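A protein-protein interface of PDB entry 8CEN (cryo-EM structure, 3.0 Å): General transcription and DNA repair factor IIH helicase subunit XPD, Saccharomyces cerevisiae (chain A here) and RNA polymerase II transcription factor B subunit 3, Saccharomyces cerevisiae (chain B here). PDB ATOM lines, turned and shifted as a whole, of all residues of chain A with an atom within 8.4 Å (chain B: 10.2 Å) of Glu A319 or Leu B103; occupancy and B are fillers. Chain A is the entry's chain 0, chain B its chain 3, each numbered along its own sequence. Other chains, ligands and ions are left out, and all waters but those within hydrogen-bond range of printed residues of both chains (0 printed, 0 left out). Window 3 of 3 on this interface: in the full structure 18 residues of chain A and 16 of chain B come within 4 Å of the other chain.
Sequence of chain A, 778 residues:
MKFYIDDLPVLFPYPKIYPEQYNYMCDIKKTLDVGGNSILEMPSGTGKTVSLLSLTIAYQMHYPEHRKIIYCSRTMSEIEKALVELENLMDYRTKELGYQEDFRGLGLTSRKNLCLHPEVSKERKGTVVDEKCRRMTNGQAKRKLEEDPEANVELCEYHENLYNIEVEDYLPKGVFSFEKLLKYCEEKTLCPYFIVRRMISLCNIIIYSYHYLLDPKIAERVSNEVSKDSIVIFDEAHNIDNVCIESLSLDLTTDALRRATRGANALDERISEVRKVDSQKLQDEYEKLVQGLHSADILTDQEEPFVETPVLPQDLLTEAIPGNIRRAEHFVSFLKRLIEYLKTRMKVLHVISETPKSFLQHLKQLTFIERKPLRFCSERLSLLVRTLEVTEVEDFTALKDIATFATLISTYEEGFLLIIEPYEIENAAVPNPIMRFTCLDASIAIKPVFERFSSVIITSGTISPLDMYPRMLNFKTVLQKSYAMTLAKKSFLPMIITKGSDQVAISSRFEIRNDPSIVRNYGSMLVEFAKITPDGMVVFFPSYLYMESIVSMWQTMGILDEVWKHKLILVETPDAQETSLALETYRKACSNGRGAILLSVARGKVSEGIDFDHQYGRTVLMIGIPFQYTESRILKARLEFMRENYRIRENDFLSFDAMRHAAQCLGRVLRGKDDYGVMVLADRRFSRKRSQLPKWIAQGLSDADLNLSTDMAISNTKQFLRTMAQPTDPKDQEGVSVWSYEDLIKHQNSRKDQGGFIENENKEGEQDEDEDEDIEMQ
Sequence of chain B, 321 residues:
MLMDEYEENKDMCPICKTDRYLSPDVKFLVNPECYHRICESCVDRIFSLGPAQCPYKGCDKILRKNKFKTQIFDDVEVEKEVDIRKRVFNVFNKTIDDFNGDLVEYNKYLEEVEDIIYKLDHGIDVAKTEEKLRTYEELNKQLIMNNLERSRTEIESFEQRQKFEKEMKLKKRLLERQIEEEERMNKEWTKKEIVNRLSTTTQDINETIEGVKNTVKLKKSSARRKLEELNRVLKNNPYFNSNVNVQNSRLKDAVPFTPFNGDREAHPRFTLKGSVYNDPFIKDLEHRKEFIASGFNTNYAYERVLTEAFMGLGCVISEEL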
ATOM      1  N   LEU A 289      10.532  -1.292 -20.855  1.00  0.00           N
ATOM      2  CA  LEU A 289      10.548  -2.728 -21.113  1.00  0.00           C
ATOM      3  C   LEU A 289       9.323  -3.417 -20.521  1.00  0.00           C
ATOM      4  O   LEU A 289       8.822  -4.393 -21.092  1.00  0.00           O
ATOM      5  CB  LEU A 289      11.834  -3.350 -20.571  1.00  0.00           C
ATOM      6  CG  LEU A 289      13.129  -2.980 -21.300  1.00  0.00           C
ATOM      7  CD1 LEU A 289      14.319  -3.726 -20.718  1.00  0.00           C
ATOM      8  CD2 LEU A 289      13.007  -3.237 -22.793  1.00  0.00           C
ATOM      9  N   GLY A 292       6.657  -2.744 -22.879  1.00  0.00           N
ATOM     10  CA  GLY A 292       6.837  -3.608 -24.025  1.00  0.00           C
ATOM     11  C   GLY A 292       7.577  -2.996 -25.191  1.00  0.00           C
ATOM     12  O   GLY A 292       7.635  -3.621 -26.257  1.00  0.00           O
ATOM     13  N   LEU A 293       8.134  -1.799 -25.034  1.00  0.00           N
ATOM     14  CA  LEU A 293       8.849  -1.152 -26.125  1.00  0.00           C
ATOM     15  C   LEU A 293      10.157  -1.878 -26.412  1.00  0.00           C
ATOM     16  O   LEU A 293      10.892  -2.261 -25.499  1.00  0.00           O
ATOM     17  CB  LEU A 293       9.114   0.315 -25.790  1.00  0.00           C
ATOM     18  CG  LEU A 293       7.896   1.143 -25.374  1.00  0.00           C
ATOM     19  CD1 LEU A 293       8.269   2.607 -25.216  1.00  0.00           C
ATOM     20  CD2 LEU A 293       6.756   0.987 -26.370  1.00  0.00           C
ATOM     21  N   HIS A 294      10.439  -2.068 -27.695  1.00  0.00           N
ATOM     22  CA  HIS A 294      11.588  -2.828 -28.150  1.00  0.00           C
ATOM     23  C   HIS A 294      12.745  -1.880 -28.460  1.00  0.00           C
ATOM     24  O   HIS A 294      12.698  -0.683 -28.152  1.00  0.00           O
ATOM     25  CB  HIS A 294      11.195  -3.671 -29.364  1.00  0.00           C
ATOM     26  CG  HIS A 294      10.553  -4.975 -29.008  1.00  0.00           C
ATOM     27  ND1 HIS A 294       9.186  -5.138 -28.951  1.00  0.00           N
ATOM     28  CD2 HIS A 294      11.088  -6.177 -28.690  1.00  0.00           C
ATOM     29  CE1 HIS A 294       8.907  -6.384 -28.613  1.00  0.00           C
ATOM     30  NE2 HIS A 294      10.043  -7.036 -28.449  1.00  0.00           N
ATOM     31  N   LEU A 316      13.178 -12.917 -35.593  1.00  0.00           N
ATOM     32  CA  LEU A 316      13.166 -12.170 -34.344  1.00  0.00           C
ATOM     33  C   LEU A 316      11.794 -12.250 -33.683  1.00  0.00           C
ATOM     34  O   LEU A 316      10.758 -12.302 -34.350  1.00  0.00           O
ATOM     35  CB  LEU A 316      13.539 -10.708 -34.588  1.00  0.00           C
ATOM     36  CG  LEU A 316      15.028 -10.360 -34.621  1.00  0.00           C
ATOM     37  CD1 LEU A 316      15.221  -8.895 -34.970  1.00  0.00           C
ATOM     38  CD2 LEU A 316      15.662 -10.672 -33.278  1.00  0.00           C
ATOM     39  N   LEU A 317      11.795 -12.259 -32.352  1.00  0.00           N
ATOM     40  CA  LEU A 317      10.557 -12.350 -31.595  1.00  0.00           C
ATOM     41  C   LEU A 317       9.921 -10.975 -31.428  1.00  0.00           C
ATOM     42  O   LEU A 317      10.607  -9.957 -31.308  1.00  0.00           O
ATOM     43  CB  LEU A 317      10.810 -12.974 -30.222  1.00  0.00           C
ATOM     44  CG  LEU A 317      10.900 -14.499 -30.151  1.00  0.00           C
ATOM     45  CD1 LEU A 317      10.933 -14.964 -28.705  1.00  0.00           C
ATOM     46  CD2 LEU A 317       9.744 -15.148 -30.896  1.00  0.00           C
ATOM     47  N   THR A 318       8.587 -10.958 -31.418  1.00  0.00           N
ATOM     48  CA  THR A 318       7.824  -9.723 -31.299  1.00  0.00           C
ATOM     49  C   THR A 318       7.277  -9.483 -29.898  1.00  0.00           C
ATOM     50  O   THR A 318       6.743  -8.401 -29.639  1.00  0.00           O
ATOM     51  CB  THR A 318       6.661  -9.719 -32.300  1.00  0.00           C
ATOM     52  OG1 THR A 318       5.779 -10.811 -32.014  1.00  0.00           O
ATOM     53  CG2 THR A 318       7.184  -9.856 -33.720  1.00  0.00           C
ATOM     54  N   GLU A 319       7.384 -10.458 -29.001  1.00  0.00           N
ATOM     55  CA  GLU A 319       6.901 -10.286 -27.641  1.00  0.00           C
ATOM     56  C   GLU A 319       7.910  -9.495 -26.810  1.00  0.00           C
ATOM     57  O   GLU A 319       9.036  -9.225 -27.234  1.00  0.00           O
ATOM     58  CB  GLU A 319       6.614 -11.640 -26.994  1.00  0.00           C
ATOM     59  CG  GLU A 319       5.408 -12.359 -27.580  1.00  0.00           C
ATOM     60  CD  GLU A 319       5.145 -13.696 -26.916  1.00  0.00           C
ATOM     61  OE1 GLU A 319       5.980 -14.131 -26.097  1.00  0.00           O
ATOM     62  OE2 GLU A 319       4.099 -14.313 -27.213  1.00  0.00           O
ATOM     63  N   ALA A 320       7.486  -9.123 -25.605  1.00  0.00           N
ATOM     64  CA  ALA A 320       8.308  -8.309 -24.726  1.00  0.00           C
ATOM     65  C   ALA A 320       9.446  -9.132 -24.122  1.00  0.00           C
ATOM     66  O   ALA A 320       9.549 -10.348 -24.315  1.00  0.00           O
ATOM     67  CB  ALA A 320       7.455  -7.693 -23.616  1.00  0.00           C
ATOM     68  N   ILE A 321      10.319  -8.437 -23.400  1.00  0.00           N
ATOM     69  CA  ILE A 321      11.433  -9.083 -22.694  1.00  0.00           C
ATOM     70  C   ILE A 321      10.873 -10.002 -21.614  1.00  0.00           C
ATOM     71  O   ILE A 321       9.945  -9.601 -20.884  1.00  0.00           O
ATOM     72  CB  ILE A 321      12.368  -8.019 -22.088  1.00  0.00           C
ATOM     73  CG1 ILE A 321      12.695  -6.944 -23.125  1.00  0.00           C
ATOM     74  CG2 ILE A 321      13.654  -8.644 -21.569  1.00  0.00           C
ATOM     75  CD1 ILE A 321      13.504  -7.446 -24.300  1.00  0.00           C
ATOM     76  N   PRO A 322      11.364 -11.240 -21.487  1.00  0.00           N
ATOM     77  CA  PRO A 322      10.776 -12.176 -20.511  1.00  0.00           C
ATOM     78  C   PRO A 322      10.941 -11.765 -19.056  1.00  0.00           C
ATOM     79  O   PRO A 322      10.211 -12.280 -18.201  1.00  0.00           O
ATOM     80  CB  PRO A 322      11.509 -13.494 -20.803  1.00  0.00           C
ATOM     81  CG  PRO A 322      12.731 -13.095 -21.565  1.00  0.00           C
ATOM     82  CD  PRO A 322      12.317 -11.919 -22.378  1.00  0.00           C
ATOM     83  N   GLY A 323      11.870 -10.873 -18.737  1.00  0.00           N
ATOM     84  CA  GLY A 323      12.013 -10.387 -17.383  1.00  0.00           C
ATOM     85  C   GLY A 323      13.159 -10.989 -16.600  1.00  0.00           C
ATOM     86  O   GLY A 323      13.492 -10.462 -15.530  1.00  0.00           O
ATOM     87  N   ARG A 326      15.592  -8.196 -17.662  1.00  0.00           N
ATOM     88  CA  ARG A 326      15.052  -6.845 -17.783  1.00  0.00           C
ATOM     89  C   ARG A 326      15.828  -5.845 -16.934  1.00  0.00           C
ATOM     90  O   ARG A 326      16.119  -4.733 -17.389  1.00  0.00           O
ATOM     91  CB  ARG A 326      13.580  -6.830 -17.393  1.00  0.00           C
ATOM     92  CG  ARG A 326      12.832  -5.603 -17.851  1.00  0.00           C
ATOM     93  CD  ARG A 326      11.353  -5.725 -17.547  1.00  0.00           C
ATOM     94  NE  ARG A 326      10.648  -6.540 -18.527  1.00  0.00           N
ATOM     95  CZ  ARG A 326       9.704  -7.418 -18.222  1.00  0.00           C
ATOM     96  NH1 ARG A 326       9.328  -7.622 -16.970  1.00  0.00           N
ATOM     97  NH2 ARG A 326       9.119  -8.108 -19.196  1.00  0.00           N
ATOM     98  N   LYS A 372      14.207 -18.346 -24.478  1.00  0.00           N
ATOM     99  CA  LYS A 372      13.594 -17.037 -24.696  1.00  0.00           C
ATOM    100  C   LYS A 372      14.403 -15.861 -24.142  1.00  0.00           C
ATOM    101  O   LYS A 372      14.507 -14.849 -24.857  1.00  0.00           O
ATOM    102  CB  LYS A 372      12.157 -17.042 -24.154  1.00  0.00           C
ATOM    103  CG  LYS A 372      11.349 -15.814 -24.533  1.00  0.00           C
ATOM    104  CD  LYS A 372       9.955 -15.866 -23.936  1.00  0.00           C
ATOM    105  CE  LYS A 372       9.103 -16.917 -24.625  1.00  0.00           C
ATOM    106  NZ  LYS A 372       7.713 -16.942 -24.092  1.00  0.00           N
ATOM    107  N   PHE A 376      16.558 -12.561 -26.728  1.00  0.00           N
ATOM    108  CA  PHE A 376      16.565 -11.111 -26.596  1.00  0.00           C
ATOM    109  C   PHE A 376      17.903 -10.570 -26.110  1.00  0.00           C
ATOM    110  O   PHE A 376      17.967  -9.413 -25.681  1.00  0.00           O
ATOM    111  CB  PHE A 376      15.459 -10.661 -25.642  1.00  0.00           C
ATOM    112  CG  PHE A 376      14.074 -10.900 -26.159  1.00  0.00           C
ATOM    113  CD1 PHE A 376      13.453  -9.964 -26.969  1.00  0.00           C
ATOM    114  CD2 PHE A 376      13.391 -12.057 -25.834  1.00  0.00           C
ATOM    115  CE1 PHE A 376      12.176 -10.181 -27.443  1.00  0.00           C
ATOM    116  CE2 PHE A 376      12.115 -12.281 -26.306  1.00  0.00           C
ATOM    117  CZ  PHE A 376      11.506 -11.342 -27.109  1.00  0.00           C
ATOM    118  N   GLU A 379      19.492  -7.525 -28.180  1.00  0.00           N
ATOM    119  CA  GLU A 379      18.658  -6.344 -27.986  1.00  0.00           C
ATOM    120  C   GLU A 379      18.815  -5.774 -26.581  1.00  0.00           C
ATOM    121  O   GLU A 379      18.923  -4.552 -26.407  1.00  0.00           O
ATOM    122  CB  GLU A 379      17.199  -6.706 -28.261  1.00  0.00           C
ATOM    123  CG  GLU A 379      16.218  -5.576 -28.056  1.00  0.00           C
ATOM    124  CD  GLU A 379      14.882  -5.856 -28.707  1.00  0.00           C
ATOM    125  OE1 GLU A 379      14.038  -6.513 -28.064  1.00  0.00           O
ATOM    126  OE2 GLU A 379      14.679  -5.431 -29.863  1.00  0.00           O
ATOM    127  N   THR B  95       5.407 -21.819 -14.322  1.00  0.00           N
ATOM    128  CA  THR B  95       5.636 -21.562 -15.737  1.00  0.00           C
ATOM    129  C   THR B  95       4.446 -20.799 -16.320  1.00  0.00           C
ATOM    130  O   THR B  95       3.530 -20.380 -15.601  1.00  0.00           O
ATOM    131  CB  THR B  95       5.879 -22.871 -16.495  1.00  0.00           C
ATOM    132  OG1 THR B  95       4.717 -23.705 -16.400  1.00  0.00           O
ATOM    133  CG2 THR B  95       7.082 -23.610 -15.925  1.00  0.00           C
ATOM    134  N   ILE B  96       4.471 -20.619 -17.643  1.00  0.00           N
ATOM    135  CA  ILE B  96       3.370 -19.946 -18.322  1.00  0.00           C
ATOM    136  C   ILE B  96       2.108 -20.806 -18.282  1.00  0.00           C
ATOM    137  O   ILE B  96       0.988 -20.280 -18.296  1.00  0.00           O
ATOM    138  CB  ILE B  96       3.789 -19.566 -19.760  1.00  0.00           C
ATOM    139  CG1 ILE B  96       2.786 -18.592 -20.386  1.00  0.00           C
ATOM    140  CG2 ILE B  96       3.995 -20.801 -20.637  1.00  0.00           C
ATOM    141  CD1 ILE B  96       2.748 -17.245 -19.704  1.00  0.00           C
ATOM    142  N   ASP B  97       2.261 -22.131 -18.197  1.00  0.00           N
ATOM    143  CA  ASP B  97       1.103 -22.999 -18.003  1.00  0.00           C
ATOM    144  C   ASP B  97       0.516 -22.824 -16.608  1.00  0.00           C
ATOM    145  O   ASP B  97      -0.705 -22.888 -16.430  1.00  0.00           O
ATOM    146  CB  ASP B  97       1.493 -24.456 -18.245  1.00  0.00           C
ATOM    147  CG  ASP B  97       1.811 -24.740 -19.699  1.00  0.00           C
ATOM    148  OD1 ASP B  97       1.240 -24.059 -20.577  1.00  0.00           O
ATOM    149  OD2 ASP B  97       2.632 -25.644 -19.964  1.00  0.00           O
ATOM    150  N   ASP B  98       1.373 -22.607 -15.607  1.00  0.00           N
ATOM    151  CA  ASP B  98       0.887 -22.347 -14.257  1.00  0.00           C
ATOM    152  C   ASP B  98       0.250 -20.968 -14.146  1.00  0.00           C
ATOM    153  O   ASP B  98      -0.654 -20.769 -13.327  1.00  0.00           O
ATOM    154  CB  ASP B  98       2.027 -22.493 -13.251  1.00  0.00           C
ATOM    155  CG  ASP B  98       2.493 -23.929 -13.103  1.00  0.00           C
ATOM    156  OD1 ASP B  98       1.667 -24.845 -13.296  1.00  0.00           O
ATOM    157  OD2 ASP B  98       3.684 -24.143 -12.796  1.00  0.00           O
ATOM    158  N   PHE B  99       0.702 -20.009 -14.951  1.00  0.00           N
ATOM    159  CA  PHE B  99       0.103 -18.681 -14.974  1.00  0.00           C
ATOM    160  C   PHE B  99      -1.009 -18.542 -16.005  1.00  0.00           C
ATOM    161  O   PHE B  99      -1.542 -17.438 -16.166  1.00  0.00           O
ATOM    162  CB  PHE B  99       1.176 -17.617 -15.222  1.00  0.00           C
ATOM    163  CG  PHE B  99       1.815 -17.105 -13.966  1.00  0.00           C
ATOM    164  CD1 PHE B  99       2.888 -17.769 -13.396  1.00  0.00           C
ATOM    165  CD2 PHE B  99       1.327 -15.969 -13.343  1.00  0.00           C
ATOM    166  CE1 PHE B  99       3.471 -17.301 -12.234  1.00  0.00           C
ATOM    167  CE2 PHE B  99       1.903 -15.495 -12.182  1.00  0.00           C
ATOM    168  CZ  PHE B  99       2.975 -16.163 -11.626  1.00  0.00           C
ATOM    169  N   ASN B 100      -1.347 -19.631 -16.707  1.00  0.00           N
ATOM    170  CA  ASN B 100      -2.485 -19.698 -17.633  1.00  0.00           C
ATOM    171  C   ASN B 100      -2.351 -18.695 -18.778  1.00  0.00           C
ATOM    172  O   ASN B 100      -3.323 -18.057 -19.188  1.00  0.00           O
ATOM    173  CB  ASN B 100      -3.817 -19.511 -16.898  1.00  0.00           C
ATOM    174  CG  ASN B 100      -4.385 -20.817 -16.380  1.00  0.00           C
ATOM    175  OD1 ASN B 100      -5.117 -21.513 -17.084  1.00  0.00           O
ATOM    176  ND2 ASN B 100      -4.046 -21.160 -15.142  1.00  0.00           N
ATOM    177  N   GLY B 101      -1.135 -18.554 -19.298  1.00  0.00           N
ATOM    178  CA  GLY B 101      -0.892 -17.713 -20.450  1.00  0.00           C
ATOM    179  C   GLY B 101      -0.764 -16.234 -20.167  1.00  0.00           C
ATOM    180  O   GLY B 101      -0.588 -15.456 -21.113  1.00  0.00           O
ATOM    181  N   ASP B 102      -0.846 -15.813 -18.908  1.00  0.00           N
ATOM    182  CA  ASP B 102      -0.722 -14.399 -18.565  1.00  0.00           C
ATOM    183  C   ASP B 102       0.748 -14.011 -18.651  1.00  0.00           C
ATOM    184  O   ASP B 102       1.523 -14.232 -17.714  1.00  0.00           O
ATOM    185  CB  ASP B 102      -1.296 -14.129 -17.180  1.00  0.00           C
ATOM    186  CG  ASP B 102      -1.786 -12.703 -17.022  1.00  0.00           C
ATOM    187  OD1 ASP B 102      -1.430 -11.854 -17.865  1.00  0.00           O
ATOM    188  OD2 ASP B 102      -2.539 -12.434 -16.062  1.00  0.00           O
ATOM    189  N   LEU B 103       1.131 -13.431 -19.792  1.00  0.00           N
ATOM    190  CA  LEU B 103       2.541 -13.175 -20.075  1.00  0.00           C
ATOM    191  C   LEU B 103       3.116 -12.108 -19.151  1.00  0.00           C
ATOM    192  O   LEU B 103       4.250 -12.243 -18.681  1.00  0.00           O
ATOM    193  CB  LEU B 103       2.713 -12.769 -21.538  1.00  0.00           C
ATOM    194  CG  LEU B 103       4.145 -12.527 -22.016  1.00  0.00           C
ATOM    195  CD1 LEU B 103       4.964 -13.804 -21.910  1.00  0.00           C
ATOM    196  CD2 LEU B 103       4.157 -11.993 -23.440  1.00  0.00           C
ATOM    197  N   VAL B 104       2.351 -11.050 -18.871  1.00  0.00           N
ATOM    198  CA  VAL B 104       2.856  -9.979 -18.015  1.00  0.00           C
ATOM    199  C   VAL B 104       3.015 -10.460 -16.575  1.00  0.00           C
ATOM    200  O   VAL B 104       3.977 -10.095 -15.887  1.00  0.00           O
ATOM    201  CB  VAL B 104       1.953  -8.733 -18.121  1.00  0.00           C
ATOM    202  CG1 VAL B 104       2.109  -8.093 -19.490  1.00  0.00           C
ATOM    203  CG2 VAL B 104       0.491  -9.089 -17.889  1.00  0.00           C
ATOM    204  N   GLU B 105       2.099 -11.311 -16.104  1.00  0.00           N
ATOM    205  CA  GLU B 105       2.237 -11.865 -14.762  1.00  0.00           C
ATOM    206  C   GLU B 105       3.390 -12.857 -14.684  1.00  0.00           C
ATOM    207  O   GLU B 105       4.069 -12.933 -13.654  1.00  0.00           O
ATOM    208  CB  GLU B 105       0.928 -12.519 -14.325  1.00  0.00           C
ATOM    209  CG  GLU B 105      -0.162 -11.520 -13.971  1.00  0.00           C
ATOM    210  CD  GLU B 105       0.012 -10.933 -12.584  1.00  0.00           C
ATOM    211  OE1 GLU B 105      -0.132 -11.683 -11.596  1.00  0.00           O
ATOM    212  OE2 GLU B 105       0.296  -9.720 -12.484  1.00  0.00           O
ATOM    213  N   TYR B 106       3.636 -13.610 -15.762  1.00  0.00           N
ATOM    214  CA  TYR B 106       4.805 -14.485 -15.796  1.00  0.00           C
ATOM    215  C   TYR B 106       6.099 -13.676 -15.784  1.00  0.00           C
ATOM    216  O   TYR B 106       7.077 -14.063 -15.127  1.00  0.00           O
ATOM    217  CB  TYR B 106       4.744 -15.390 -17.026  1.00  0.00           C
ATOM    218  CG  TYR B 106       5.888 -16.374 -17.126  1.00  0.00           C
ATOM    219  CD1 TYR B 106       6.081 -17.340 -16.148  1.00  0.00           C
ATOM    220  CD2 TYR B 106       6.770 -16.341 -18.199  1.00  0.00           C
ATOM    221  CE1 TYR B 106       7.122 -18.246 -16.232  1.00  0.00           C
ATOM    222  CE2 TYR B 106       7.814 -17.242 -18.292  1.00  0.00           C
ATOM    223  CZ  TYR B 106       7.985 -18.192 -17.306  1.00  0.00           C
ATOM    224  OH  TYR B 106       9.021 -19.093 -17.394  1.00  0.00           O
ATOM    225  N   ASN B 107       6.116 -12.544 -16.494  1.00  0.00           N
ATOM    226  CA  ASN B 107       7.277 -11.659 -16.461  1.00  0.00           C
ATOM    227  C   ASN B 107       7.490 -11.083 -15.066  1.00  0.00           C
ATOM    228  O   ASN B 107       8.631 -10.975 -14.604  1.00  0.00           O
ATOM    229  CB  ASN B 107       7.123 -10.529 -17.481  1.00  0.00           C
ATOM    230  CG  ASN B 107       7.017 -11.031 -18.908  1.00  0.00           C
ATOM    231  OD1 ASN B 107       7.615 -12.042 -19.272  1.00  0.00           O
ATOM    232  ND2 ASN B 107       6.254 -10.319 -19.728  1.00  0.00           N
ATOM    233  N   LYS B 108       6.404 -10.716 -14.379  1.00  0.00           N
ATOM    234  CA  LYS B 108       6.527 -10.193 -13.020  1.00  0.00           C
ATOM    235  C   LYS B 108       7.017 -11.268 -12.053  1.00  0.00           C
ATOM    236  O   LYS B 108       7.797 -10.978 -11.134  1.00  0.00           O
ATOM    237  CB  LYS B 108       5.190  -9.610 -12.559  1.00  0.00           C
ATOM    238  CG  LYS B 108       5.229  -8.939 -11.192  1.00  0.00           C
ATOM    239  CD  LYS B 108       3.867  -8.383 -10.807  1.00  0.00           C
ATOM    240  CE  LYS B 108       3.895  -7.756  -9.422  1.00  0.00           C
ATOM    241  NZ  LYS B 108       2.555  -7.248  -9.016  1.00  0.00           N
ATOM    242  N   TYR B 109       6.580 -12.516 -12.249  1.00  0.00           N
ATOM    243  CA  TYR B 109       7.098 -13.613 -11.436  1.00  0.00           C
ATOM    244  C   TYR B 109       8.589 -13.810 -11.677  1.00  0.00           C
ATOM    245  O   TYR B 109       9.346 -14.064 -10.733  1.00  0.00           O
ATOM    246  CB  TYR B 109       6.299 -14.898 -11.709  1.00  0.00           C
ATOM    247  CG  TYR B 109       6.855 -16.187 -11.108  1.00  0.00           C
ATOM    248  CD1 TYR B 109       7.873 -16.915 -11.733  1.00  0.00           C
ATOM    249  CD2 TYR B 109       6.256 -16.751  -9.990  1.00  0.00           C
ATOM    250  CE1 TYR B 109       8.345 -18.095 -11.195  1.00  0.00           C
ATOM    251  CE2 TYR B 109       6.730 -17.928  -9.439  1.00  0.00           C
ATOM    252  CZ  TYR B 109       7.768 -18.600 -10.051  1.00  0.00           C
ATOM    253  OH  TYR B 109       8.230 -19.781  -9.520  1.00  0.00           O
ATOM    254  N   LEU B 110       9.024 -13.712 -12.936  1.00  0.00           N
ATOM    255  CA  LEU B 110      10.450 -13.811 -13.229  1.00  0.00           C
ATOM    256  C   LEU B 110      11.223 -12.655 -12.600  1.00  0.00           C
ATOM    257  O   LEU B 110      12.355 -12.840 -12.133  1.00  0.00           O
ATOM    258  CB  LEU B 110      10.670 -13.869 -14.740  1.00  0.00           C
ATOM    259  CG  LEU B 110      10.228 -15.193 -15.371  1.00  0.00           C
ATOM    260  CD1 LEU B 110      10.584 -15.263 -16.844  1.00  0.00           C
ATOM    261  CD2 LEU B 110      10.838 -16.369 -14.618  1.00  0.00           C
ATOM    262  N   GLU B 111      10.615 -11.464 -12.556  1.00  0.00           N
ATOM    263  CA  GLU B 111      11.214 -10.339 -11.839  1.00  0.00           C
ATOM    264  C   GLU B 111      11.407 -10.665 -10.365  1.00  0.00           C
ATOM    265  O   GLU B 111      12.475 -10.409  -9.801  1.00  0.00           O
ATOM    266  CB  GLU B 111      10.349  -9.083 -11.978  1.00  0.00           C
ATOM    267  CG  GLU B 111      10.254  -8.514 -13.372  1.00  0.00           C
ATOM    268  CD  GLU B 111      11.568  -7.968 -13.868  1.00  0.00           C
ATOM    269  OE1 GLU B 111      12.368  -7.470 -13.045  1.00  0.00           O
ATOM    270  OE2 GLU B 111      11.803  -8.050 -15.085  1.00  0.00           O
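O of Pro A322 lies close to OD1 of Asn B107 (2.8 Å).
NH1 of Arg A326 is in salt-bridge range of OE2 of Glu B111 (3.1 Å).
The backbone carbonyl oxygen of Gly A323 sits close to the side-chain carboxylate of Glu B111.
NE2 of His A294 sits at hydrogen-bond distance from O of Glu A319, at 2.7 Å.
The side-chain carboxylate (OE1) of Glu A319 is in salt-bridge range of the side-chain amino group (NZ) of Lys A372 (3.9 Å).
The backbone carbonyl oxygen (O) of Ile A321 sits at hydrogen-bond distance from the guanidinium group (NH2) of Arg A326, 2.4 Å away.
The backbone carbonyl oxygen of Leu B103 sits at hydrogen-bond distance from the side-chain amide nitrogen of Asn B107.
Among the printed residues, merely in contact across the chains: Glu A319 with Leu B103, Ile A321 with Asn B107, Pro A322 with Leu B110 and Arg A326 with Asn B107.
Of chain B, only Leu B103 (3.9 Å) comes within 4 Å of Glu A319.
Leu B103 touches just one residue of chain A: Glu A319.
Ala A320 touches none of the printed residues of chain B.
No residue of chain A comes within 4 Å of Val B104.
Of the printed residues of chain A, Leu B110 touches Pro A322 (3.3 Å).
Of the printed residues of chain B, Ile A321 touches Asn B107 (3.7 Å).
The nearest residue of chain A that does not touch Leu B103 is Lys A372 (4.7 Å).
The nearest printed residue of chain B that does not touch Ile A321 is Glu B111 (6.3 Å).
Printed residues of chain A that touch a printed residue of chain B: Glu A319, Ile A321, Pro A322, Gly A323 and Arg A326.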
